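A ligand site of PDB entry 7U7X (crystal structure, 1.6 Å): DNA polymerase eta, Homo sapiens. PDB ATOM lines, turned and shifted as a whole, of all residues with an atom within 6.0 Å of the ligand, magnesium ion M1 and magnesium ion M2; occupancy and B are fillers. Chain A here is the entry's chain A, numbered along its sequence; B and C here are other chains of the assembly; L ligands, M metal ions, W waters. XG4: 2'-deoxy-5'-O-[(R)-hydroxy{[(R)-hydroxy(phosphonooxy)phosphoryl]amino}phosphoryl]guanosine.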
ATOM      1  N   ASP A  16      -7.156  -3.843  16.971  1.00  0.00           N
ATOM      2  CA  ASP A  16      -8.628  -3.727  16.909  1.00  0.00           C
ATOM      3  C   ASP A  16      -9.210  -4.778  15.972  1.00  0.00           C
ATOM      4  O   ASP A  16      -8.795  -4.865  14.833  1.00  0.00           O
ATOM      5  CB  ASP A  16      -9.070  -2.338  16.447  1.00  0.00           C
ATOM      6  CG  ASP A  16     -10.558  -2.112  16.571  1.00  0.00           C
ATOM      7  OD1 ASP A  16     -11.278  -2.503  15.658  1.00  0.00           O
ATOM      8  OD2 ASP A  16     -10.965  -1.533  17.569  1.00  0.00           O
ATOM      9  N   MET A  17     -10.182  -5.522  16.474  1.00  0.00           N
ATOM     10  CA  MET A  17     -10.813  -6.561  15.648  1.00  0.00           C
ATOM     11  C   MET A  17     -11.627  -5.922  14.512  1.00  0.00           C
ATOM     12  O   MET A  17     -12.340  -4.983  14.755  1.00  0.00           O
ATOM     13  CB  MET A  17     -11.696  -7.478  16.506  1.00  0.00           C
ATOM     14  CG  MET A  17     -11.016  -7.949  17.765  1.00  0.00           C
ATOM     15  SD  MET A  17      -9.519  -8.878  17.420  1.00  0.00           S
ATOM     16  CE  MET A  17     -10.167 -10.151  16.356  1.00  0.00           C
ATOM     17  N   ASP A  18     -11.482  -6.424  13.300  1.00  0.00           N
ATOM     18  CA  ASP A  18     -12.274  -5.915  12.156  1.00  0.00           C
ATOM     19  C   ASP A  18     -13.757  -6.306  12.336  1.00  0.00           C
ATOM     20  O   ASP A  18     -13.980  -7.455  12.661  1.00  0.00           O
ATOM     21  CB  ASP A  18     -11.731  -6.515  10.850  1.00  0.00           C
ATOM     22  CG  ASP A  18     -10.273  -6.217  10.605  1.00  0.00           C
ATOM     23  OD1 ASP A  18      -9.811  -5.149  11.023  1.00  0.00           O
ATOM     24  OD2 ASP A  18      -9.596  -7.050   9.999  1.00  0.00           O
ATOM     25  N   CYS A  19     -14.684  -5.390  12.085  1.00  0.00           N
ATOM     26  CA  CYS A  19     -16.164  -5.639  12.184  1.00  0.00           C
ATOM     27  C   CYS A  19     -16.387  -6.771  13.193  1.00  0.00           C
ATOM     28  O   CYS A  19     -16.940  -7.774  12.785  1.00  0.00           O
ATOM     29  CB  CYS A  19     -16.731  -5.913  10.792  1.00  0.00           C
ATOM     30  SG  CYS A  19     -15.903  -7.160   9.768  1.00  0.00           S
ATOM     31  N   PHE A  20     -16.140  -6.510  14.487  1.00  0.00           N
ATOM     32  CA  PHE A  20     -15.990  -7.634  15.425  1.00  0.00           C
ATOM     33  C   PHE A  20     -17.263  -8.486  15.541  1.00  0.00           C
ATOM     34  O   PHE A  20     -17.204  -9.709  15.351  1.00  0.00           O
ATOM     35  CB  PHE A  20     -15.575  -7.123  16.802  1.00  0.00           C
ATOM     36  CG  PHE A  20     -15.303  -8.235  17.795  1.00  0.00           C
ATOM     37  CD1 PHE A  20     -14.532  -9.321  17.437  1.00  0.00           C
ATOM     38  CD2 PHE A  20     -15.829  -8.175  19.079  1.00  0.00           C
ATOM     39  CE1 PHE A  20     -14.282 -10.363  18.366  1.00  0.00           C
ATOM     40  CE2 PHE A  20     -15.592  -9.193  19.989  1.00  0.00           C
ATOM     41  CZ  PHE A  20     -14.814 -10.283  19.626  1.00  0.00           C
ATOM     42  N   PHE A  21     -18.395  -7.875  15.888  1.00  0.00           N
ATOM     43  CA  PHE A  21     -19.604  -8.686  16.088  1.00  0.00           C
ATOM     44  C   PHE A  21     -19.972  -9.443  14.806  1.00  0.00           C
ATOM     45  O   PHE A  21     -20.506 -10.571  14.868  1.00  0.00           O
ATOM     46  CB  PHE A  21     -20.787  -7.838  16.552  1.00  0.00           C
ATOM     47  CG  PHE A  21     -20.708  -7.317  17.967  1.00  0.00           C
ATOM     48  CD1 PHE A  21     -19.514  -7.255  18.684  1.00  0.00           C
ATOM     49  CD2 PHE A  21     -21.880  -6.871  18.590  1.00  0.00           C
ATOM     50  CE1 PHE A  21     -19.486  -6.731  19.982  1.00  0.00           C
ATOM     51  CE2 PHE A  21     -21.861  -6.355  19.900  1.00  0.00           C
ATOM     52  CZ  PHE A  21     -20.654  -6.285  20.592  1.00  0.00           C
ATOM     53  N   VAL A  22     -19.760  -8.821  13.636  1.00  0.00           N
ATOM     54  CA  VAL A  22     -19.978  -9.530  12.366  1.00  0.00           C
ATOM     55  C   VAL A  22     -19.084 -10.760  12.279  1.00  0.00           C
ATOM     56  O   VAL A  22     -19.559 -11.840  11.909  1.00  0.00           O
ATOM     57  CB  VAL A  22     -19.740  -8.588  11.172  1.00  0.00           C
ATOM     58  CG1 VAL A  22     -19.626  -9.363   9.864  1.00  0.00           C
ATOM     59  CG2 VAL A  22     -20.861  -7.568  11.079  1.00  0.00           C
ATOM     60  N   GLN A  41     -29.466  -4.881  16.555  1.00  0.00           N
ATOM     61  CA  GLN A  41     -30.186  -5.190  17.787  1.00  0.00           C
ATOM     62  C   GLN A  41     -31.648  -4.801  17.616  1.00  0.00           C
ATOM     63  O   GLN A  41     -31.963  -3.710  17.118  1.00  0.00           O
ATOM     64  CB  GLN A  41     -29.512  -4.615  19.039  1.00  0.00           C
ATOM     65  CG  GLN A  41     -28.973  -3.245  18.999  1.00  0.00           C
ATOM     66  CD  GLN A  41     -27.922  -2.937  20.116  1.00  0.00           C
ATOM     67  OE1 GLN A  41     -27.400  -3.818  20.862  1.00  0.00           O
ATOM     68  NE2 GLN A  41     -27.628  -1.678  20.221  1.00  0.00           N
ATOM     69  N   ILE A  51     -25.227  -2.212  14.406  1.00  0.00           N
ATOM     70  CA  ILE A  51     -24.076  -1.847  15.242  1.00  0.00           C
ATOM     71  C   ILE A  51     -22.745  -2.346  14.701  1.00  0.00           C
ATOM     72  O   ILE A  51     -21.687  -1.958  15.246  1.00  0.00           O
ATOM     73  CB  ILE A  51     -24.256  -2.323  16.700  1.00  0.00           C
ATOM     74  CG1 ILE A  51     -24.572  -3.821  16.759  1.00  0.00           C
ATOM     75  CG2 ILE A  51     -25.338  -1.487  17.420  1.00  0.00           C
ATOM     76  CD1 ILE A  51     -24.513  -4.356  18.188  1.00  0.00           C
ATOM     77  N   ALA A  52     -22.720  -3.154  13.633  1.00  0.00           N
ATOM     78  CA  ALA A  52     -21.467  -3.648  13.070  1.00  0.00           C
ATOM     79  C   ALA A  52     -21.728  -4.039  11.617  1.00  0.00           C
ATOM     80  O   ALA A  52     -22.804  -4.550  11.310  1.00  0.00           O
ATOM     81  CB  ALA A  52     -20.899  -4.836  13.860  1.00  0.00           C
ATOM     82  N   VAL A  53     -20.744  -3.784  10.739  1.00  0.00           N
ATOM     83  CA  VAL A  53     -20.939  -3.861   9.289  1.00  0.00           C
ATOM     84  C   VAL A  53     -19.703  -4.485   8.641  1.00  0.00           C
ATOM     85  O   VAL A  53     -18.590  -3.974   8.812  1.00  0.00           O
ATOM     86  CB  VAL A  53     -21.206  -2.463   8.692  1.00  0.00           C
ATOM     87  CG1 VAL A  53     -21.541  -2.564   7.188  1.00  0.00           C
ATOM     88  CG2 VAL A  53     -22.300  -1.732   9.453  1.00  0.00           C
ATOM     89  N   TYR A  55     -17.007  -5.368   5.687  1.00  0.00           N
ATOM     90  CA  TYR A  55     -16.399  -4.433   4.737  1.00  0.00           C
ATOM     91  C   TYR A  55     -17.063  -4.519   3.353  1.00  0.00           C
ATOM     92  O   TYR A  55     -17.192  -3.496   2.658  1.00  0.00           O
ATOM     93  CB  TYR A  55     -14.884  -4.684   4.672  1.00  0.00           C
ATOM     94  CG  TYR A  55     -14.243  -4.034   5.877  1.00  0.00           C
ATOM     95  CD1 TYR A  55     -14.310  -4.627   7.125  1.00  0.00           C
ATOM     96  CD2 TYR A  55     -13.614  -2.792   5.776  1.00  0.00           C
ATOM     97  CE1 TYR A  55     -13.757  -4.016   8.247  1.00  0.00           C
ATOM     98  CE2 TYR A  55     -13.064  -2.177   6.890  1.00  0.00           C
ATOM     99  CZ  TYR A  55     -13.138  -2.787   8.121  1.00  0.00           C
ATOM    100  OH  TYR A  55     -12.591  -2.159   9.241  1.00  0.00           O
ATOM    101  N   ARG A  58     -20.019  -2.305   3.818  1.00  0.00           N
ATOM    102  CA  ARG A  58     -19.594  -0.902   3.856  1.00  0.00           C
ATOM    103  C   ARG A  58     -19.421  -0.327   2.469  1.00  0.00           C
ATOM    104  O   ARG A  58     -19.642   0.872   2.261  1.00  0.00           O
ATOM    105  CB  ARG A  58     -18.285  -0.756   4.642  1.00  0.00           C
ATOM    106  CG  ARG A  58     -18.400  -1.167   6.111  1.00  0.00           C
ATOM    107  CD  ARG A  58     -17.078  -0.964   6.797  1.00  0.00           C
ATOM    108  NE  ARG A  58     -17.085  -1.548   8.128  1.00  0.00           N
ATOM    109  CZ  ARG A  58     -16.198  -1.239   9.059  1.00  0.00           C
ATOM    110  NH1 ARG A  58     -15.220  -0.388   8.815  1.00  0.00           N
ATOM    111  NH2 ARG A  58     -16.280  -1.814  10.251  1.00  0.00           N
ATOM    112  N   ARG A  64     -22.721   1.707  10.815  1.00  0.00           N
ATOM    113  CA  ARG A  64     -23.197   1.759  12.180  1.00  0.00           C
ATOM    114  C   ARG A  64     -24.227   2.874  12.324  1.00  0.00           C
ATOM    115  O   ARG A  64     -24.105   3.922  11.692  1.00  0.00           O
ATOM    116  CB  ARG A  64     -21.976   1.977  13.073  1.00  0.00           C
ATOM    117  CG  ARG A  64     -22.211   1.940  14.513  1.00  0.00           C
ATOM    118  CD  ARG A  64     -21.063   2.634  15.236  1.00  0.00           C
ATOM    119  NE  ARG A  64     -21.527   2.931  16.573  1.00  0.00           N
ATOM    120  CZ  ARG A  64     -21.977   4.114  16.947  1.00  0.00           C
ATOM    121  NH1 ARG A  64     -21.814   5.183  16.186  1.00  0.00           N
ATOM    122  NH2 ARG A  64     -22.606   4.233  18.114  1.00  0.00           N
ATOM    123  N   LEU A  92     -25.377  -9.318  25.214  1.00  0.00           N
ATOM    124  CA  LEU A  92     -24.151  -9.319  24.421  1.00  0.00           C
ATOM    125  C   LEU A  92     -23.136 -10.361  24.895  1.00  0.00           C
ATOM    126  O   LEU A  92     -21.945 -10.253  24.569  1.00  0.00           O
ATOM    127  CB  LEU A  92     -23.534  -7.920  24.418  1.00  0.00           C
ATOM    128  CG  LEU A  92     -24.484  -6.796  23.998  1.00  0.00           C
ATOM    129  CD1 LEU A  92     -23.824  -5.437  24.147  1.00  0.00           C
ATOM    130  CD2 LEU A  92     -24.968  -7.025  22.599  1.00  0.00           C
ATOM    131  N   SER A 116     -11.600  -1.686  24.943  1.00  0.00           N
ATOM    132  CA  SER A 116     -13.021  -1.880  24.566  1.00  0.00           C
ATOM    133  C   SER A 116     -13.257  -3.370  24.427  1.00  0.00           C
ATOM    134  O   SER A 116     -12.303  -4.106  24.567  1.00  0.00           O
ATOM    135  CB  SER A 116     -13.342  -1.217  23.253  1.00  0.00           C
ATOM    136  OG  SER A 116     -13.025  -2.060  22.179  1.00  0.00           O
ATOM    137  N   ILE A 117     -14.472  -3.758  24.036  1.00  0.00           N
ATOM    138  CA  ILE A 117     -14.777  -5.187  23.789  1.00  0.00           C
ATOM    139  C   ILE A 117     -13.920  -5.732  22.637  1.00  0.00           C
ATOM    140  O   ILE A 117     -13.734  -6.935  22.564  1.00  0.00           O
ATOM    141  CB  ILE A 117     -16.279  -5.379  23.485  1.00  0.00           C
ATOM    142  CG1 ILE A 117     -16.743  -6.812  23.700  1.00  0.00           C
ATOM    143  CG2 ILE A 117     -16.659  -4.859  22.112  1.00  0.00           C
ATOM    144  CD1 ILE A 117     -18.245  -6.956  23.748  1.00  0.00           C
ATOM    145  N   ASP A 118     -13.401  -4.865  21.779  1.00  0.00           N
ATOM    146  CA  ASP A 118     -12.713  -5.406  20.588  1.00  0.00           C
ATOM    147  C   ASP A 118     -11.297  -4.859  20.425  1.00  0.00           C
ATOM    148  O   ASP A 118     -10.677  -5.139  19.403  1.00  0.00           O
ATOM    149  CB  ASP A 118     -13.582  -5.214  19.350  1.00  0.00           C
ATOM    150  CG  ASP A 118     -13.278  -3.955  18.563  1.00  0.00           C
ATOM    151  OD1 ASP A 118     -13.121  -2.897  19.174  1.00  0.00           O
ATOM    152  OD2 ASP A 118     -13.183  -4.092  17.334  1.00  0.00           O
ATOM    153  N   GLU A 119     -10.791  -4.138  21.415  1.00  0.00           N
ATOM    154  CA  GLU A 119      -9.442  -3.587  21.189  1.00  0.00           C
ATOM    155  C   GLU A 119      -8.621  -3.508  22.463  1.00  0.00           C
ATOM    156  O   GLU A 119      -9.185  -3.355  23.545  1.00  0.00           O
ATOM    157  CB  GLU A 119      -9.464  -2.231  20.522  1.00  0.00           C
ATOM    158  CG  GLU A 119      -9.915  -1.108  21.403  1.00  0.00           C
ATOM    159  CD  GLU A 119     -10.599  -0.053  20.559  1.00  0.00           C
ATOM    160  OE1 GLU A 119     -11.698  -0.319  20.075  1.00  0.00           O
ATOM    161  OE2 GLU A 119     -10.045   1.043  20.474  1.00  0.00           O
ATOM    162  N   LYS A 227      -3.432   4.073  17.822  1.00  0.00           N
ATOM    163  CA  LYS A 227      -4.850   3.970  17.461  1.00  0.00           C
ATOM    164  C   LYS A 227      -5.108   4.581  16.085  1.00  0.00           C
ATOM    165  O   LYS A 227      -5.775   3.973  15.217  1.00  0.00           O
ATOM    166  CB  LYS A 227      -5.693   4.673  18.535  1.00  0.00           C
ATOM    167  CG  LYS A 227      -7.206   4.755  18.263  1.00  0.00           C
ATOM    168  CD  LYS A 227      -7.844   3.366  18.208  1.00  0.00           C
ATOM    169  CE  LYS A 227      -9.385   3.459  18.120  1.00  0.00           C
ATOM    170  NZ  LYS A 227     -10.080   2.115  18.005  1.00  0.00           N
ATOM    171  N   LYS A 234      -7.224  -0.560   7.598  1.00  0.00           N
ATOM    172  CA  LYS A 234      -8.183  -1.623   7.834  1.00  0.00           C
ATOM    173  C   LYS A 234      -8.835  -2.035   6.514  1.00  0.00           C
ATOM    174  O   LYS A 234      -9.088  -1.192   5.652  1.00  0.00           O
ATOM    175  CB  LYS A 234      -9.262  -1.113   8.798  1.00  0.00           C
ATOM    176  CG  LYS A 234      -8.915  -1.252  10.285  1.00  0.00           C
ATOM    177  CD  LYS A 234     -10.133  -1.097  11.190  1.00  0.00           C
ATOM    178  CE  LYS A 234      -9.846  -1.683  12.589  1.00  0.00           C
ATOM    179  NZ  LYS A 234     -10.515  -3.003  12.804  1.00  0.00           N
ATOM    180  N   PRO A 235      -9.220  -3.323   6.354  1.00  0.00           N
ATOM    181  CA  PRO A 235      -9.133  -4.434   7.302  1.00  0.00           C
ATOM    182  C   PRO A 235      -7.926  -5.344   7.132  1.00  0.00           C
ATOM    183  O   PRO A 235      -7.285  -5.370   6.071  1.00  0.00           O
ATOM    184  CB  PRO A 235     -10.413  -5.236   7.005  1.00  0.00           C
ATOM    185  CG  PRO A 235     -10.534  -5.099   5.487  1.00  0.00           C
ATOM    186  CD  PRO A 235     -10.041  -3.691   5.177  1.00  0.00           C
ATOM    187  P    DT B   3     -33.941   8.441  16.372  1.00  0.00           P
ATOM    188  OP1  DT B   3     -34.228   9.791  16.923  1.00  0.00           O
ATOM    189  OP2  DT B   3     -33.713   8.257  14.931  1.00  0.00           O
ATOM    190  O5'  DT B   3     -32.688   7.853  17.154  1.00  0.00           O
ATOM    191  C5'  DT B   3     -31.827   6.958  16.460  1.00  0.00           C
ATOM    192  C4'  DT B   3     -31.886   5.589  17.075  1.00  0.00           C
ATOM    193  O4'  DT B   3     -30.750   4.821  16.598  1.00  0.00           O
ATOM    194  C3'  DT B   3     -31.801   5.556  18.598  1.00  0.00           C
ATOM    195  O3'  DT B   3     -32.677   4.551  19.106  1.00  0.00           O
ATOM    196  C2'  DT B   3     -30.336   5.276  18.887  1.00  0.00           C
ATOM    197  C1'  DT B   3     -29.757   4.699  17.598  1.00  0.00           C
ATOM    198  N1   DT B   3     -28.547   5.398  17.134  1.00  0.00           N
ATOM    199  C2   DT B   3     -27.334   4.767  17.251  1.00  0.00           C
ATOM    200  O2   DT B   3     -27.214   3.637  17.702  1.00  0.00           O
ATOM    201  N3   DT B   3     -26.258   5.506  16.830  1.00  0.00           N
ATOM    202  C4   DT B   3     -26.284   6.774  16.279  1.00  0.00           C
ATOM    203  O4   DT B   3     -25.235   7.316  15.925  1.00  0.00           O
ATOM    204  C5   DT B   3     -27.583   7.380  16.190  1.00  0.00           C
ATOM    205  C7   DT B   3     -27.712   8.753  15.603  1.00  0.00           C
ATOM    206  C6   DT B   3     -28.634   6.672  16.625  1.00  0.00           C
ATOM    207  P    DT B   4     -32.799   4.305  20.675  1.00  0.00           P
ATOM    208  OP1  DT B   4     -34.142   3.730  20.946  1.00  0.00           O
ATOM    209  OP2  DT B   4     -32.353   5.525  21.381  1.00  0.00           O
ATOM    210  O5'  DT B   4     -31.735   3.162  20.928  1.00  0.00           O
ATOM    211  C5'  DT B   4     -31.814   1.907  20.230  1.00  0.00           C
ATOM    212  C4'  DT B   4     -30.910   0.900  20.901  1.00  0.00           C
ATOM    213  O4'  DT B   4     -29.540   1.117  20.470  1.00  0.00           O
ATOM    214  C3'  DT B   4     -30.884   0.962  22.421  1.00  0.00           C
ATOM    215  O3'  DT B   4     -30.831  -0.379  22.891  1.00  0.00           O
ATOM    216  C2'  DT B   4     -29.605   1.728  22.725  1.00  0.00           C
ATOM    217  C1'  DT B   4     -28.699   1.317  21.586  1.00  0.00           C
ATOM    218  N1   DT B   4     -27.683   2.298  21.206  1.00  0.00           N
ATOM    219  C2   DT B   4     -26.430   1.833  20.893  1.00  0.00           C
ATOM    220  O2   DT B   4     -26.132   0.651  20.931  1.00  0.00           O
ATOM    221  N3   DT B   4     -25.531   2.801  20.523  1.00  0.00           N
ATOM    222  C4   DT B   4     -25.759   4.162  20.437  1.00  0.00           C
ATOM    223  O4   DT B   4     -24.861   4.914  20.091  1.00  0.00           O
ATOM    224  C5   DT B   4     -27.100   4.583  20.770  1.00  0.00           C
ATOM    225  C7   DT B   4     -27.435   6.038  20.727  1.00  0.00           C
ATOM    226  C6   DT B   4     -27.987   3.644  21.135  1.00  0.00           C
ATOM    227  P    DA B   5     -30.853  -0.752  24.429  1.00  0.00           P
ATOM    228  OP1  DA B   5     -31.733  -1.903  24.614  1.00  0.00           O
ATOM    229  OP2  DA B   5     -31.053   0.448  25.277  1.00  0.00           O
ATOM    230  O5'  DA B   5     -29.368  -1.265  24.688  1.00  0.00           O
ATOM    231  C5'  DA B   5     -28.723  -2.187  23.809  1.00  0.00           C
ATOM    232  C4'  DA B   5     -27.300  -2.397  24.255  1.00  0.00           C
ATOM    233  O4'  DA B   5     -26.486  -1.300  23.780  1.00  0.00           O
ATOM    234  C3'  DA B   5     -27.125  -2.425  25.773  1.00  0.00           C
ATOM    235  O3'  DA B   5     -26.160  -3.422  26.160  1.00  0.00           O
ATOM    236  C2'  DA B   5     -26.625  -1.034  26.105  1.00  0.00           C
ATOM    237  C1'  DA B   5     -25.822  -0.679  24.867  1.00  0.00           C
ATOM    238  N9   DA B   5     -25.786   0.749  24.620  1.00  0.00           N
ATOM    239  C8   DA B   5     -26.771   1.675  24.874  1.00  0.00           C
ATOM    240  N7   DA B   5     -26.437   2.899  24.543  1.00  0.00           N
ATOM    241  C5   DA B   5     -25.159   2.771  24.036  1.00  0.00           C
ATOM    242  C6   DA B   5     -24.255   3.703  23.507  1.00  0.00           C
ATOM    243  N6   DA B   5     -24.507   5.010  23.407  1.00  0.00           N
ATOM    244  N1   DA B   5     -23.051   3.250  23.091  1.00  0.00           N
ATOM    245  C2   DA B   5     -22.788   1.936  23.194  1.00  0.00           C
ATOM    246  N3   DA B   5     -23.554   0.964  23.667  1.00  0.00           N
ATOM    247  C4   DA B   5     -24.741   1.455  24.080  1.00  0.00           C
ATOM    248  P    DT C   8     -14.474   6.186  18.275  1.00  0.00           P
ATOM    249  OP1  DT C   8     -13.158   5.677  17.855  1.00  0.00           O
ATOM    250  OP2  DT C   8     -15.081   7.334  17.591  1.00  0.00           O
ATOM    251  O5'  DT C   8     -15.491   4.966  18.172  1.00  0.00           O
ATOM    252  C5'  DT C   8     -15.396   3.809  19.013  1.00  0.00           C
ATOM    253  C4'  DT C   8     -16.668   3.005  18.843  1.00  0.00           C
ATOM    254  O4'  DT C   8     -17.647   3.455  19.806  1.00  0.00           O
ATOM    255  C3'  DT C   8     -17.311   3.190  17.463  1.00  0.00           C
ATOM    256  O3'  DT C   8     -17.853   1.957  16.973  1.00  0.00           O
ATOM    257  C2'  DT C   8     -18.493   4.088  17.758  1.00  0.00           C
ATOM    258  C1'  DT C   8     -18.873   3.572  19.123  1.00  0.00           C
ATOM    259  N1   DT C   8     -19.758   4.463  19.861  1.00  0.00           N
ATOM    260  C2   DT C   8     -20.511   3.915  20.871  1.00  0.00           C
ATOM    261  O2   DT C   8     -20.393   2.754  21.227  1.00  0.00           O
ATOM    262  N3   DT C   8     -21.390   4.779  21.464  1.00  0.00           N
ATOM    263  C4   DT C   8     -21.603   6.099  21.140  1.00  0.00           C
ATOM    264  O4   DT C   8     -22.428   6.758  21.772  1.00  0.00           O
ATOM    265  C5   DT C   8     -20.803   6.608  20.055  1.00  0.00           C
ATOM    266  C7   DT C   8     -20.965   8.031  19.635  1.00  0.00           C
ATOM    267  C6   DT C   8     -19.946   5.767  19.471  1.00  0.00           C
HETATM  268  N1  XG4 L   1     -23.839  -0.319  20.692  1.00  0.00           N
HETATM  269  C2  XG4 L   1     -23.448  -1.617  20.934  1.00  0.00           C
HETATM  270  N2  XG4 L   1     -24.273  -2.341  21.698  1.00  0.00           N
HETATM  271  N3  XG4 L   1     -22.353  -2.203  20.437  1.00  0.00           N
HETATM  272  C4  XG4 L   1     -21.618  -1.410  19.663  1.00  0.00           C
HETATM  273  C5  XG4 L   1     -21.884  -0.120  19.361  1.00  0.00           C
HETATM  274  C6  XG4 L   1     -23.057   0.435  19.902  1.00  0.00           C
HETATM  275  O6  XG4 L   1     -23.383   1.617  19.686  1.00  0.00           O
HETATM  276  N7  XG4 L   1     -20.928   0.388  18.489  1.00  0.00           N
HETATM  277  C8  XG4 L   1     -20.104  -0.627  18.292  1.00  0.00           C
HETATM  278  N9  XG4 L   1     -20.472  -1.748  18.981  1.00  0.00           N
HETATM  279  PA  XG4 L   1     -15.556  -1.140  16.629  1.00  0.00           P
HETATM  280  PB  XG4 L   1     -15.890  -2.904  14.304  1.00  0.00           P
HETATM  281  PG  XG4 L   1     -13.828  -1.934  12.638  1.00  0.00           P
HETATM  282  C1' XG4 L   1     -19.855  -3.072  18.978  1.00  0.00           C
HETATM  283  O1A XG4 L   1     -14.141  -1.511  16.793  1.00  0.00           O
HETATM  284  O1B XG4 L   1     -15.052  -3.831  15.088  1.00  0.00           O
HETATM  285  O1G XG4 L   1     -13.084  -1.878  13.912  1.00  0.00           O
HETATM  286  C2' XG4 L   1     -19.979  -3.777  17.631  1.00  0.00           C
HETATM  287  O2A XG4 L   1     -15.761   0.446  16.739  1.00  0.00           O
HETATM  288  O2B XG4 L   1     -17.279  -3.499  14.019  1.00  0.00           O
HETATM  289  O2G XG4 L   1     -13.235  -2.925  11.657  1.00  0.00           O
HETATM  290  C3' XG4 L   1     -18.561  -3.720  17.061  1.00  0.00           C
HETATM  291  O3' XG4 L   1     -18.368  -4.891  16.276  1.00  0.00           O
HETATM  292  N3A XG4 L   1     -16.171  -1.565  15.180  1.00  0.00           N
HETATM  293  O3B XG4 L   1     -15.296  -2.456  12.918  1.00  0.00           O
HETATM  294  O3G XG4 L   1     -14.021  -0.554  11.952  1.00  0.00           O
HETATM  295  C4' XG4 L   1     -17.703  -3.709  18.323  1.00  0.00           C
HETATM  296  O4' XG4 L   1     -18.466  -2.926  19.265  1.00  0.00           O
HETATM  297  C5' XG4 L   1     -16.316  -3.101  18.188  1.00  0.00           C
HETATM  298  O5' XG4 L   1     -16.450  -1.721  17.783  1.00  0.00           O
HETATM  299 MG    MG M   1     -12.810  -1.027  18.524  1.00  0.00          MG
HETATM  300 MG    MG M   2     -13.023  -3.185  15.567  1.00  0.00          MG
HETATM  301  O   HOH W   1     -18.998  -0.657  14.769  1.00  0.00           O
HETATM  302  O   HOH W   2     -14.454  -0.484  19.807  1.00  0.00           O
HETATM  303  O   HOH W   3     -18.553  -2.462  11.966  1.00  0.00           O
HETATM  304  O   HOH W   4     -11.959   0.448  14.789  1.00  0.00           O
HETATM  305  O   HOH W   5     -12.688   0.843  17.439  1.00  0.00           O
HETATM  306  O   HOH W   6     -15.993   1.050  12.256  1.00  0.00           O
HETATM  307  O   HOH W   7     -17.321  -0.878  20.744  1.00  0.00           O
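N of Cys 19 lies within hydrogen-bond range of O2G of the ligand, at 2.9 Å.
NH2 of Arg 64 lies within hydrogen-bond range of O6 of the ligand, 3.1 Å away.
N3 of DA 5 of chain B is in hydrogen-bond range of N1 of the ligand, at 3.3 Å.
A nitrogen (N2) of the ligand sits at hydrogen-bond distance from O4' of DA 5 of chain B (3.2 Å).
O3' of DT 8 of chain C sits close to O2A of the ligand (2.6 Å).
O2 of DT 4 of chain B lies within hydrogen-bond range of a nitrogen (N1) of the ligand (2.5 Å).
N of Phe 21 sits at hydrogen-bond distance from O3' of the ligand (3.0 Å).
O2G of the ligand lies within salt-bridge range of NZ of Lys 234 (3.0 Å).
The guanidinium group (NH2) of Arg 58 lies within salt-bridge range of an oxygen (O3G) of the ligand, 3.1 Å away.
O2B of the ligand sits at hydrogen-bond distance from N of Phe 20, 3.3 Å away.
The side-chain hydroxyl (OH) of Tyr 55 sits at hydrogen-bond distance from an oxygen (O2G) of the ligand (2.6 Å).
The side-chain amino group (NZ) of Lys 234 sits close to the backbone carbonyl oxygen (O) of Met 17, at 3.3 Å.
The side-chain amino group (NZ) of Lys 234 lies within salt-bridge range of the side-chain carboxylate (OD1) of Asp 18 (2.9 Å).
The backbone carbonyl oxygen (O) of Val 53 sits at hydrogen-bond distance from the guanidinium group (NE) of Arg 58 (2.9 Å).
N of Glu 119 is in hydrogen-bond range of OG of Ser 116 (3.1 Å).
N of Asp 118 sits at hydrogen-bond distance from OG of Ser 116 (2.9 Å).
O2 of DT 4 of chain B lies within hydrogen-bond range of NE2 of Gln 41 (2.9 Å).
The side-chain amino group of Lys 227 sits close to the side-chain carboxylate of Asp 16.
The guanidinium group (NH2) of Arg 64 lies within hydrogen-bond range of N1 of DT 8 of chain C (3.3 Å).
Merely in contact with the ligand: Asp 18 (3.2 Å), Ile 51 (3.5 Å), Ala 52 (3.5 Å), Gln 41 (3.6 Å), Ile 117 (3.9 Å) and Leu 92 (3.97 Å).
Hydrophobic or aromatic side chains that line the ligand: Phe 20, Phe 21, Ile 51, Ala 52, Tyr 55, Leu 92 and Ile 117.
19 residues have an atom within 4 Å of the ligand: Asp 16, Met 17, Asp 18, Cys 19, Phe 20, Phe 21, Gln 41, Ile 51, Ala 52, Tyr 55, Arg 58, Arg 64, Leu 92, Ile 117, Asp 118, Lys 234, DT 4 of chain B, DA 5 of chain B and DT 8 of chain C.
The nearest printed residue that does not touch the ligand is Glu 119 (4.3 Å).
Ser 116 touches magnesium ion M1 (OG to MG, 3.8 Å).
Four residues have an atom within 4 Å of magnesium ion M1: Asp 16, Ser 116, Asp 118 and Glu 119.
The nearest printed residue that does not touch magnesium ion M1 is Lys 227 (4.2 Å).
Lys 234 touches magnesium ion M2 (NZ to MG, 3.7 Å).
Four residues have an atom within 4 Å of magnesium ion M2: Asp 16, Met 17, Asp 118 and Lys 234.
The nearest printed residue that does not touch magnesium ion M2 is Asp 18 (4.2 Å).
Magnesium ion M1 is bound by the side-chain carboxylate of Asp 118 (2.0 Å), the side-chain carboxylate of Glu 119 (2.0 Å), the side-chain carboxylate of Asp 16 (2.1 Å), water W2 (2.2 Å), water W5 (2.2 Å) and an oxygen (O1A) of the ligand (2.2 Å).
Magnesium ion M2 is bound by the side-chain carboxylate of Asp 16 (1.9 Å), the side-chain carboxylate of Asp 118 (2.0 Å), the backbone carbonyl oxygen of Met 17 (2.1 Å), an oxygen (O1G) of the ligand (2.1 Å), an oxygen (O1B) of the ligand (2.2 Å) and an oxygen (O1A) of the ligand (2.4 Å).
Water W2 lies within hydrogen-bond range of O5' of the ligand and OG of Ser 116.
Water W5 bridges NZ of Lys 227 (3.0 Å) and O2A of the ligand (3.2 Å).
Water W3 lies within hydrogen-bond range of O2B of the ligand (2.6 Å), N of Val 53 (2.8 Å) and NH2 of Arg 58 (2.9 Å).
Water W1 bridges N3A of the ligand and O of Ile 51.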
